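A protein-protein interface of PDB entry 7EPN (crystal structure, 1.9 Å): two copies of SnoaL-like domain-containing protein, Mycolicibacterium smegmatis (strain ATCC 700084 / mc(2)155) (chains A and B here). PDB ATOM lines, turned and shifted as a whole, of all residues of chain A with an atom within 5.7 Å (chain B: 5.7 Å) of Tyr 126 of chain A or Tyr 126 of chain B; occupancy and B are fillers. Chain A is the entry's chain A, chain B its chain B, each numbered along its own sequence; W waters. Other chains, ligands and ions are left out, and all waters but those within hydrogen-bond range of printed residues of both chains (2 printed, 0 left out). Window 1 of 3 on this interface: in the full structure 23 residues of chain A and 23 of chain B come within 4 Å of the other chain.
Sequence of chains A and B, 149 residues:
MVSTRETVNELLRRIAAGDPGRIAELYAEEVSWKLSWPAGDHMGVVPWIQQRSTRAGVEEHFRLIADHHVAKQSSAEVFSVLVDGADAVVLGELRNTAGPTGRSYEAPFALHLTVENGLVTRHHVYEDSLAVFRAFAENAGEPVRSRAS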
ATOM      1  N   LYS A  34       8.013   9.560  -2.069  1.00  0.00           N
ATOM      2  CA  LYS A  34       7.227  10.531  -1.320  1.00  0.00           C
ATOM      3  C   LYS A  34       7.545  11.919  -1.850  1.00  0.00           C
ATOM      4  O   LYS A  34       8.681  12.194  -2.254  1.00  0.00           O
ATOM      5  CB  LYS A  34       7.516  10.447   0.188  1.00  0.00           C
ATOM      6  CG  LYS A  34       6.977  11.586   1.046  1.00  0.00           C
ATOM      7  CD  LYS A  34       7.175  11.249   2.520  1.00  0.00           C
ATOM      8  CE  LYS A  34       6.472  12.224   3.454  1.00  0.00           C
ATOM      9  NZ  LYS A  34       6.889  12.027   4.891  1.00  0.00           N
ATOM     10  N   SER A  36       6.647  16.212  -1.044  1.00  0.00           N
ATOM     11  CA  SER A  36       6.141  17.189  -0.078  1.00  0.00           C
ATOM     12  C   SER A  36       5.021  18.036  -0.695  1.00  0.00           C
ATOM     13  O   SER A  36       5.126  19.256  -0.819  1.00  0.00           O
ATOM     14  CB  SER A  36       7.283  18.055   0.438  1.00  0.00           C
ATOM     15  OG  SER A  36       7.740  18.924  -0.584  1.00  0.00           O
ATOM     16  N   PHE A  79      23.748  22.014  -4.491  1.00  0.00           N
ATOM     17  CA  PHE A  79      24.618  22.713  -3.543  1.00  0.00           C
ATOM     18  C   PHE A  79      25.429  21.757  -2.675  1.00  0.00           C
ATOM     19  O   PHE A  79      26.624  21.987  -2.455  1.00  0.00           O
ATOM     20  CB  PHE A  79      23.789  23.630  -2.630  1.00  0.00           C
ATOM     21  CG  PHE A  79      23.018  24.684  -3.380  1.00  0.00           C
ATOM     22  CD1 PHE A  79      23.675  25.526  -4.263  1.00  0.00           C
ATOM     23  CD2 PHE A  79      21.646  24.826  -3.205  1.00  0.00           C
ATOM     24  CE1 PHE A  79      22.979  26.508  -4.969  1.00  0.00           C
ATOM     25  CE2 PHE A  79      20.936  25.802  -3.901  1.00  0.00           C
ATOM     26  CZ  PHE A  79      21.606  26.647  -4.787  1.00  0.00           C
ATOM     27  N   LEU A  91      20.885  18.505  -1.707  1.00  0.00           N
ATOM     28  CA  LEU A  91      20.308  19.835  -1.545  1.00  0.00           C
ATOM     29  C   LEU A  91      20.608  20.669  -2.785  1.00  0.00           C
ATOM     30  O   LEU A  91      21.741  20.676  -3.276  1.00  0.00           O
ATOM     31  CB  LEU A  91      20.870  20.517  -0.296  1.00  0.00           C
ATOM     32  CG  LEU A  91      20.692  19.645   0.949  1.00  0.00           C
ATOM     33  CD1 LEU A  91      21.702  20.027   2.007  1.00  0.00           C
ATOM     34  CD2 LEU A  91      19.262  19.753   1.470  1.00  0.00           C
ATOM     35  N   GLY A  92      19.597  21.358  -3.296  1.00  0.00           N
ATOM     36  CA  GLY A  92      19.800  22.120  -4.509  1.00  0.00           C
ATOM     37  C   GLY A  92      18.608  22.999  -4.826  1.00  0.00           C
ATOM     38  O   GLY A  92      17.775  23.284  -3.964  1.00  0.00           O
ATOM     39  N   PRO A 108      13.788  25.548  -4.371  1.00  0.00           N
ATOM     40  CA  PRO A 108      14.766  24.776  -3.599  1.00  0.00           C
ATOM     41  C   PRO A 108      14.217  23.390  -3.322  1.00  0.00           C
ATOM     42  O   PRO A 108      13.006  23.197  -3.147  1.00  0.00           O
ATOM     43  CB  PRO A 108      14.928  25.578  -2.298  1.00  0.00           C
ATOM     44  CG  PRO A 108      14.278  26.898  -2.534  1.00  0.00           C
ATOM     45  CD  PRO A 108      13.288  26.726  -3.641  1.00  0.00           C
ATOM     46  N   PHE A 109      15.116  22.410  -3.294  1.00  0.00           N
ATOM     47  CA  PHE A 109      14.691  21.055  -3.005  1.00  0.00           C
ATOM     48  C   PHE A 109      15.732  20.363  -2.145  1.00  0.00           C
ATOM     49  O   PHE A 109      16.919  20.707  -2.164  1.00  0.00           O
ATOM     50  CB  PHE A 109      14.446  20.245  -4.296  1.00  0.00           C
ATOM     51  CG  PHE A 109      15.702  19.915  -5.040  1.00  0.00           C
ATOM     52  CD1 PHE A 109      16.446  18.785  -4.710  1.00  0.00           C
ATOM     53  CD2 PHE A 109      16.155  20.734  -6.062  1.00  0.00           C
ATOM     54  CE1 PHE A 109      17.618  18.484  -5.385  1.00  0.00           C
ATOM     55  CE2 PHE A 109      17.319  20.431  -6.739  1.00  0.00           C
ATOM     56  CZ  PHE A 109      18.050  19.309  -6.394  1.00  0.00           C
ATOM     57  N   ALA A 110      15.247  19.408  -1.366  1.00  0.00           N
ATOM     58  CA  ALA A 110      16.056  18.437  -0.641  1.00  0.00           C
ATOM     59  C   ALA A 110      15.564  17.060  -1.068  1.00  0.00           C
ATOM     60  O   ALA A 110      14.379  16.754  -0.913  1.00  0.00           O
ATOM     61  CB  ALA A 110      15.910  18.614   0.872  1.00  0.00           C
ATOM     62  N   LEU A 111      16.453  16.250  -1.635  1.00  0.00           N
ATOM     63  CA  LEU A 111      16.097  14.916  -2.111  1.00  0.00           C
ATOM     64  C   LEU A 111      16.716  13.874  -1.185  1.00  0.00           C
ATOM     65  O   LEU A 111      17.941  13.701  -1.168  1.00  0.00           O
ATOM     66  CB  LEU A 111      16.551  14.715  -3.551  1.00  0.00           C
ATOM     67  CG  LEU A 111      16.439  13.286  -4.092  1.00  0.00           C
ATOM     68  CD1 LEU A 111      14.977  12.792  -4.054  1.00  0.00           C
ATOM     69  CD2 LEU A 111      17.028  13.212  -5.495  1.00  0.00           C
ATOM     70  N   HIS A 112      15.870  13.175  -0.426  1.00  0.00           N
ATOM     71  CA  HIS A 112      16.340  12.152   0.495  1.00  0.00           C
ATOM     72  C   HIS A 112      16.348  10.800  -0.209  1.00  0.00           C
ATOM     73  O   HIS A 112      15.305  10.338  -0.687  1.00  0.00           O
ATOM     74  CB  HIS A 112      15.463  12.105   1.748  1.00  0.00           C
ATOM     75  CG  HIS A 112      15.789  10.961   2.658  1.00  0.00           C
ATOM     76  ND1 HIS A 112      14.826  10.266   3.360  1.00  0.00           N
ATOM     77  CD2 HIS A 112      16.974  10.381   2.972  1.00  0.00           C
ATOM     78  CE1 HIS A 112      15.403   9.310   4.072  1.00  0.00           C
ATOM     79  NE2 HIS A 112      16.706   9.359   3.854  1.00  0.00           N
ATOM     80  N   HIS A 124      12.490  10.522  -1.630  1.00  0.00           N
ATOM     81  CA  HIS A 124      11.560  11.406  -0.936  1.00  0.00           C
ATOM     82  C   HIS A 124      11.972  12.844  -1.220  1.00  0.00           C
ATOM     83  O   HIS A 124      13.058  13.262  -0.812  1.00  0.00           O
ATOM     84  CB  HIS A 124      11.576  11.152   0.575  1.00  0.00           C
ATOM     85  CG  HIS A 124      11.038   9.813   0.972  1.00  0.00           C
ATOM     86  ND1 HIS A 124      10.902   9.429   2.290  1.00  0.00           N
ATOM     87  CD2 HIS A 124      10.603   8.766   0.228  1.00  0.00           C
ATOM     88  CE1 HIS A 124      10.407   8.203   2.340  1.00  0.00           C
ATOM     89  NE2 HIS A 124      10.219   7.778   1.103  1.00  0.00           N
ATOM     90  N   VAL A 125      11.106  13.599  -1.901  1.00  0.00           N
ATOM     91  CA  VAL A 125      11.424  14.952  -2.356  1.00  0.00           C
ATOM     92  C   VAL A 125      10.746  15.965  -1.444  1.00  0.00           C
ATOM     93  O   VAL A 125       9.544  15.857  -1.150  1.00  0.00           O
ATOM     94  CB  VAL A 125      10.993  15.166  -3.817  1.00  0.00           C
ATOM     95  CG1 VAL A 125      11.370  16.566  -4.280  1.00  0.00           C
ATOM     96  CG2 VAL A 125      11.635  14.122  -4.705  1.00  0.00           C
ATOM     97  N   TYR A 126      11.517  16.948  -0.996  1.00  0.00           N
ATOM     98  CA  TYR A 126      11.025  18.054  -0.186  1.00  0.00           C
ATOM     99  C   TYR A 126      11.331  19.332  -0.947  1.00  0.00           C
ATOM    100  O   TYR A 126      12.498  19.642  -1.197  1.00  0.00           O
ATOM    101  CB  TYR A 126      11.694  18.078   1.191  1.00  0.00           C
ATOM    102  CG  TYR A 126      11.564  16.805   1.973  1.00  0.00           C
ATOM    103  CD1 TYR A 126      12.378  15.707   1.702  1.00  0.00           C
ATOM    104  CD2 TYR A 126      10.644  16.705   3.003  1.00  0.00           C
ATOM    105  CE1 TYR A 126      12.257  14.542   2.437  1.00  0.00           C
ATOM    106  CE2 TYR A 126      10.519  15.558   3.746  1.00  0.00           C
ATOM    107  CZ  TYR A 126      11.318  14.476   3.463  1.00  0.00           C
ATOM    108  OH  TYR A 126      11.173  13.336   4.217  1.00  0.00           O
ATOM    109  N   GLU A 127      10.295  20.063  -1.335  1.00  0.00           N
ATOM    110  CA  GLU A 127      10.504  21.190  -2.234  1.00  0.00           C
ATOM    111  C   GLU A 127       9.415  22.230  -2.025  1.00  0.00           C
ATOM    112  O   GLU A 127       8.429  21.990  -1.323  1.00  0.00           O
ATOM    113  CB  GLU A 127      10.515  20.729  -3.700  1.00  0.00           C
ATOM    114  CG  GLU A 127       9.190  20.137  -4.148  1.00  0.00           C
ATOM    115  CD  GLU A 127       9.240  19.534  -5.546  1.00  0.00           C
ATOM    116  OE1 GLU A 127      10.332  19.503  -6.159  1.00  0.00           O
ATOM    117  OE2 GLU A 127       8.181  19.081  -6.033  1.00  0.00           O
ATOM    118  N   ASP A 128       9.585  23.386  -2.683  1.00  0.00           N
ATOM    119  CA  ASP A 128       8.618  24.492  -2.592  1.00  0.00           C
ATOM    120  C   ASP A 128       7.402  24.186  -3.464  1.00  0.00           C
ATOM    121  O   ASP A 128       7.262  24.672  -4.587  1.00  0.00           O
ATOM    122  CB  ASP A 128       9.264  25.806  -3.007  1.00  0.00           C
ATOM    123  CG  ASP A 128       8.388  27.015  -2.707  1.00  0.00           C
ATOM    124  OD1 ASP A 128       7.178  26.840  -2.427  1.00  0.00           O
ATOM    125  OD2 ASP A 128       8.923  28.141  -2.766  1.00  0.00           O
ATOM    126  N   LYS B  34      16.808  30.022   5.403  1.00  0.00           N
ATOM    127  CA  LYS B  34      16.094  29.911   4.140  1.00  0.00           C
ATOM    128  C   LYS B  34      14.877  29.025   4.310  1.00  0.00           C
ATOM    129  O   LYS B  34      14.908  28.052   5.066  1.00  0.00           O
ATOM    130  CB  LYS B  34      16.991  29.369   3.027  1.00  0.00           C
ATOM    131  CG  LYS B  34      17.902  30.437   2.427  1.00  0.00           C
ATOM    132  CD  LYS B  34      19.019  29.851   1.561  1.00  0.00           C
ATOM    133  CE  LYS B  34      18.695  28.450   1.025  1.00  0.00           C
ATOM    134  NZ  LYS B  34      17.436  28.314   0.221  1.00  0.00           N
ATOM    135  N   SER B  36      11.669  27.175   1.928  1.00  0.00           N
ATOM    136  CA  SER B  36      11.235  26.781   0.590  1.00  0.00           C
ATOM    137  C   SER B  36       9.843  27.349   0.292  1.00  0.00           C
ATOM    138  O   SER B  36       8.857  26.628   0.119  1.00  0.00           O
ATOM    139  CB  SER B  36      11.275  25.263   0.460  1.00  0.00           C
ATOM    140  OG  SER B  36      10.299  24.665   1.296  1.00  0.00           O
ATOM    141  N   PHE B  79      11.528  11.725  11.845  1.00  0.00           N
ATOM    142  CA  PHE B  79      11.726  10.350  11.394  1.00  0.00           C
ATOM    143  C   PHE B  79      13.187   9.928  11.432  1.00  0.00           C
ATOM    144  O   PHE B  79      13.489   8.776  11.762  1.00  0.00           O
ATOM    145  CB  PHE B  79      11.201  10.166   9.972  1.00  0.00           C
ATOM    146  CG  PHE B  79       9.735  10.461   9.832  1.00  0.00           C
ATOM    147  CD1 PHE B  79       8.828   9.996  10.772  1.00  0.00           C
ATOM    148  CD2 PHE B  79       9.270  11.229   8.779  1.00  0.00           C
ATOM    149  CE1 PHE B  79       7.470  10.273  10.655  1.00  0.00           C
ATOM    150  CE2 PHE B  79       7.906  11.505   8.652  1.00  0.00           C
ATOM    151  CZ  PHE B  79       7.015  11.031   9.593  1.00  0.00           C
ATOM    152  N   LEU B  91      14.710  14.898   9.084  1.00  0.00           N
ATOM    153  CA  LEU B  91      13.591  14.500   8.241  1.00  0.00           C
ATOM    154  C   LEU B  91      12.388  14.194   9.117  1.00  0.00           C
ATOM    155  O   LEU B  91      12.485  13.373  10.036  1.00  0.00           O
ATOM    156  CB  LEU B  91      13.949  13.276   7.400  1.00  0.00           C
ATOM    157  CG  LEU B  91      15.153  13.494   6.492  1.00  0.00           C
ATOM    158  CD1 LEU B  91      15.592  12.184   5.920  1.00  0.00           C
ATOM    159  CD2 LEU B  91      14.768  14.472   5.388  1.00  0.00           C
ATOM    160  N   GLY B  92      11.256  14.814   8.814  1.00  0.00           N
ATOM    161  CA  GLY B  92      10.087  14.605   9.640  1.00  0.00           C
ATOM    162  C   GLY B  92       8.813  15.112   9.001  1.00  0.00           C
ATOM    163  O   GLY B  92       8.734  15.300   7.788  1.00  0.00           O
ATOM    164  N   PRO B 108       5.341  17.291   5.305  1.00  0.00           N
ATOM    165  CA  PRO B 108       6.698  16.735   5.347  1.00  0.00           C
ATOM    166  C   PRO B 108       7.722  17.851   5.278  1.00  0.00           C
ATOM    167  O   PRO B 108       7.526  18.864   4.597  1.00  0.00           O
ATOM    168  CB  PRO B 108       6.761  15.837   4.100  1.00  0.00           C
ATOM    169  CG  PRO B 108       5.312  15.543   3.765  1.00  0.00           C
ATOM    170  CD  PRO B 108       4.574  16.800   4.148  1.00  0.00           C
ATOM    171  N   PHE B 109       8.824  17.672   5.996  1.00  0.00           N
ATOM    172  CA  PHE B 109       9.861  18.681   5.963  1.00  0.00           C
ATOM    173  C   PHE B 109      11.218  18.007   6.043  1.00  0.00           C
ATOM    174  O   PHE B 109      11.371  16.936   6.639  1.00  0.00           O
ATOM    175  CB  PHE B 109       9.695  19.708   7.112  1.00  0.00           C
ATOM    176  CG  PHE B 109      10.059  19.172   8.470  1.00  0.00           C
ATOM    177  CD1 PHE B 109      11.371  19.225   8.931  1.00  0.00           C
ATOM    178  CD2 PHE B 109       9.082  18.620   9.297  1.00  0.00           C
ATOM    179  CE1 PHE B 109      11.705  18.716  10.181  1.00  0.00           C
ATOM    180  CE2 PHE B 109       9.409  18.124  10.548  1.00  0.00           C
ATOM    181  CZ  PHE B 109      10.729  18.170  10.988  1.00  0.00           C
ATOM    182  N   ALA B 110      12.206  18.684   5.473  1.00  0.00           N
ATOM    183  CA  ALA B 110      13.612  18.382   5.674  1.00  0.00           C
ATOM    184  C   ALA B 110      14.269  19.669   6.153  1.00  0.00           C
ATOM    185  O   ALA B 110      14.080  20.730   5.550  1.00  0.00           O
ATOM    186  CB  ALA B 110      14.271  17.892   4.383  1.00  0.00           C
ATOM    187  N   LEU B 111      14.975  19.600   7.268  1.00  0.00           N
ATOM    188  CA  LEU B 111      15.582  20.789   7.854  1.00  0.00           C
ATOM    189  C   LEU B 111      17.082  20.591   7.795  1.00  0.00           C
ATOM    190  O   LEU B 111      17.611  19.711   8.475  1.00  0.00           O
ATOM    191  CB  LEU B 111      15.109  20.994   9.294  1.00  0.00           C
ATOM    192  CG  LEU B 111      15.967  21.931  10.163  1.00  0.00           C
ATOM    193  CD1 LEU B 111      15.975  23.342   9.621  1.00  0.00           C
ATOM    194  CD2 LEU B 111      15.421  21.930  11.579  1.00  0.00           C
ATOM    195  N   HIS B 112      17.762  21.407   6.998  1.00  0.00           N
ATOM    196  CA  HIS B 112      19.203  21.297   6.803  1.00  0.00           C
ATOM    197  C   HIS B 112      19.887  22.296   7.727  1.00  0.00           C
ATOM    198  O   HIS B 112      19.621  23.498   7.646  1.00  0.00           O
ATOM    199  CB  HIS B 112      19.560  21.568   5.337  1.00  0.00           C
ATOM    200  CG  HIS B 112      21.033  21.650   5.075  1.00  0.00           C
ATOM    201  ND1 HIS B 112      21.585  22.526   4.162  1.00  0.00           N
ATOM    202  CD2 HIS B 112      22.070  20.959   5.604  1.00  0.00           C
ATOM    203  CE1 HIS B 112      22.898  22.372   4.140  1.00  0.00           C
ATOM    204  NE2 HIS B 112      23.219  21.420   5.002  1.00  0.00           N
ATOM    205  N   HIS B 124      18.010  25.838   6.898  1.00  0.00           N
ATOM    206  CA  HIS B 124      17.318  25.875   5.616  1.00  0.00           C
ATOM    207  C   HIS B 124      16.210  24.837   5.669  1.00  0.00           C
ATOM    208  O   HIS B 124      16.484  23.642   5.855  1.00  0.00           O
ATOM    209  CB  HIS B 124      18.267  25.590   4.444  1.00  0.00           C
ATOM    210  CG  HIS B 124      19.310  26.648   4.233  1.00  0.00           C
ATOM    211  ND1 HIS B 124      20.271  26.556   3.251  1.00  0.00           N
ATOM    212  CD2 HIS B 124      19.549  27.810   4.888  1.00  0.00           C
ATOM    213  CE1 HIS B 124      21.053  27.621   3.302  1.00  0.00           C
ATOM    214  NE2 HIS B 124      20.641  28.396   4.291  1.00  0.00           N
ATOM    215  N   VAL B 125      14.966  25.298   5.531  1.00  0.00           N
ATOM    216  CA  VAL B 125      13.776  24.455   5.669  1.00  0.00           C
ATOM    217  C   VAL B 125      13.223  24.141   4.289  1.00  0.00           C
ATOM    218  O   VAL B 125      12.963  25.059   3.499  1.00  0.00           O
ATOM    219  CB  VAL B 125      12.703  25.160   6.511  1.00  0.00           C
ATOM    220  CG1 VAL B 125      11.419  24.318   6.535  1.00  0.00           C
ATOM    221  CG2 VAL B 125      13.222  25.442   7.906  1.00  0.00           C
ATOM    222  N   TYR B 126      13.003  22.855   4.009  1.00  0.00           N
ATOM    223  CA  TYR B 126      12.341  22.400   2.787  1.00  0.00           C
ATOM    224  C   TYR B 126      11.050  21.715   3.218  1.00  0.00           C
ATOM    225  O   TYR B 126      11.084  20.591   3.731  1.00  0.00           O
ATOM    226  CB  TYR B 126      13.223  21.436   1.991  1.00  0.00           C
ATOM    227  CG  TYR B 126      14.582  21.984   1.644  1.00  0.00           C
ATOM    228  CD1 TYR B 126      15.610  21.992   2.578  1.00  0.00           C
ATOM    229  CD2 TYR B 126      14.842  22.486   0.371  1.00  0.00           C
ATOM    230  CE1 TYR B 126      16.856  22.481   2.255  1.00  0.00           C
ATOM    231  CE2 TYR B 126      16.080  22.974   0.038  1.00  0.00           C
ATOM    232  CZ  TYR B 126      17.087  22.971   0.989  1.00  0.00           C
ATOM    233  OH  TYR B 126      18.325  23.473   0.665  1.00  0.00           O
ATOM    234  N   GLU B 127       9.912  22.378   3.024  1.00  0.00           N
ATOM    235  CA  GLU B 127       8.658  21.840   3.534  1.00  0.00           C
ATOM    236  C   GLU B 127       7.549  22.041   2.507  1.00  0.00           C
ATOM    237  O   GLU B 127       7.674  22.837   1.570  1.00  0.00           O
ATOM    238  CB  GLU B 127       8.277  22.510   4.859  1.00  0.00           C
ATOM    239  CG  GLU B 127       7.915  23.970   4.641  1.00  0.00           C
ATOM    240  CD  GLU B 127       7.705  24.740   5.926  1.00  0.00           C
ATOM    241  OE1 GLU B 127       8.160  24.281   6.992  1.00  0.00           O
ATOM    242  OE2 GLU B 127       7.078  25.809   5.859  1.00  0.00           O
ATOM    243  N   ASP B 128       6.442  21.321   2.716  1.00  0.00           N
ATOM    244  CA  ASP B 128       5.262  21.395   1.843  1.00  0.00           C
ATOM    245  C   ASP B 128       4.560  22.737   2.046  1.00  0.00           C
ATOM    246  O   ASP B 128       3.577  22.855   2.783  1.00  0.00           O
ATOM    247  CB  ASP B 128       4.331  20.223   2.142  1.00  0.00           C
ATOM    248  CG  ASP B 128       3.157  20.139   1.190  1.00  0.00           C
ATOM    249  OD1 ASP B 128       2.923  21.094   0.426  1.00  0.00           O
ATOM    250  OD2 ASP B 128       2.474  19.097   1.188  1.00  0.00           O
HETATM  251  O   HOH W   1       9.227  13.317   5.963  1.00  0.00           O
HETATM  252  O   HOH W   2      18.718  24.484  -1.705  1.00  0.00           O
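Among the printed residues, pairs that only touch across the chains: Phe 109 of chain A with Tyr 126 of chain B, His 112 of chain A with Leu 91 of chain B, Leu 91 of chain A with His 112 of chain B, Tyr 126 of chain A with Phe 109 of chain B, Tyr 126 of chain A with Ala 110 of chain B, Lys 34 of chain A with Pro 108 of chain B, Ala 110 of chain A with Tyr 126 of chain B, Tyr 126 of chain A with Tyr 126 of chain B, Pro 108 of chain A with Tyr 126 of chain B, Leu 91 of chain A with Tyr 126 of chain B, Tyr 126 of chain A with Pro 108 of chain B, Tyr 126 of chain A with Leu 91 of chain B, Lys 34 of chain A with Phe 79 of chain B and Ala 110 of chain A with Ala 110 of chain B.
Printed residues of chain B within 4 Å of Ser 36 of chain A: Asp 128 (2.9 Å).
Of the printed residues of chain B, Leu 91 of chain A touches His 112 and Tyr 126.
Printed residues of chain B within 4 Å of Ala 110 of chain A: Ala 110 and Tyr 126.
Tyr 126 of chain A touches just these residues of chain B: Leu 91, Pro 108, Phe 109, Ala 110 and Tyr 126.
Of the printed residues of chain A, Pro 108 of chain B touches Lys 34 (3.5 Å) and Tyr 126 (3.8 Å).
Of the printed residues of chain A, Tyr 126 of chain B touches Leu 91, Pro 108, Phe 109, Ala 110 and Tyr 126.
The nearest residue of chain B that does not touch Tyr 126 of chain A is Gly 92 of chain B (4.4 Å).
The nearest residue of chain A that does not touch Tyr 126 of chain B is Gly 92 of chain A (4.4 Å).
Lys 34 of chain A touches Pro 108 of chain B, but with the chains exchanged Pro 108 of chain A does not touch Lys 34 of chain B (4.4 Å).
Ser 36 of chain A touches Asp 128 of chain B, and with the chains exchanged Asp 128 of chain A touches Ser 36 of chain B.
Phe 109 of chain A touches Tyr 126 of chain B, and with the chains exchanged Tyr 126 of chain A touches Phe 109 of chain B.
Ala 110 of chain A touches Tyr 126 of chain B, and with the chains exchanged Tyr 126 of chain A touches Ala 110 of chain B.
The backbone NH (N) of Phe 79 of chain A sits at hydrogen-bond distance from the backbone carbonyl oxygen (O) of Leu 91 of chain A, 2.7 Å away.
O of Gly 92 of chain A sits at hydrogen-bond distance from N of Phe 109 of chain A, at 2.9 Å.
N of Ala 110 of chain A lies within hydrogen-bond range of O of Tyr 126 of chain A (2.8 Å).
The backbone carbonyl oxygen of His 124 of chain A sits at hydrogen-bond distance from the backbone NH of His 112 of chain A (2.8 Å).
The side-chain hydroxyl (OG) of Ser 36 of chain B is in hydrogen-bond range of the backbone NH (N) of Glu 127 of chain B (2.9 Å).
The backbone NH of Ala 110 of chain B lies within hydrogen-bond range of the backbone carbonyl oxygen of Tyr 126 of chain B, 2.8 Å away.
Water W2 bridges the side-chain hydroxyl of Tyr 126 of chain B and the backbone carbonyl oxygen of Gly 92 of chain A.
Water W1 lies within hydrogen-bond range of the side-chain hydroxyl (OH) of Tyr 126 of chain A (2.6 Å), the backbone carbonyl oxygen (O) of Gly 92 of chain B (2.7 Å) and the side-chain amino group (NZ) of Lys 34 of chain A (2.9 Å).
O of Ser 36 of chain A sits close to OD1 of Asp 128 of chain B, at 3.1 Å.
The backbone carbonyl oxygen of Glu 127 of chain A lies close to the backbone carbonyl oxygen of Glu 127 of chain B (3.1 Å).
OD1 of Asp 128 of chain A lies close to O of Ser 36 of chain B (3.1 Å).
Hydrophobic or aromatic side chains of chain A that line the printed part of chain B: Leu 91, Pro 108, Ala 110, His 112 and Tyr 126.
Of the 15 printed residues of chain B, 10 touch a printed residue of chain A.
Among the printed residues, no Asp or Glu carboxylate lies within 4 Å of a Lys or Arg side-chain nitrogen of the other chain.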
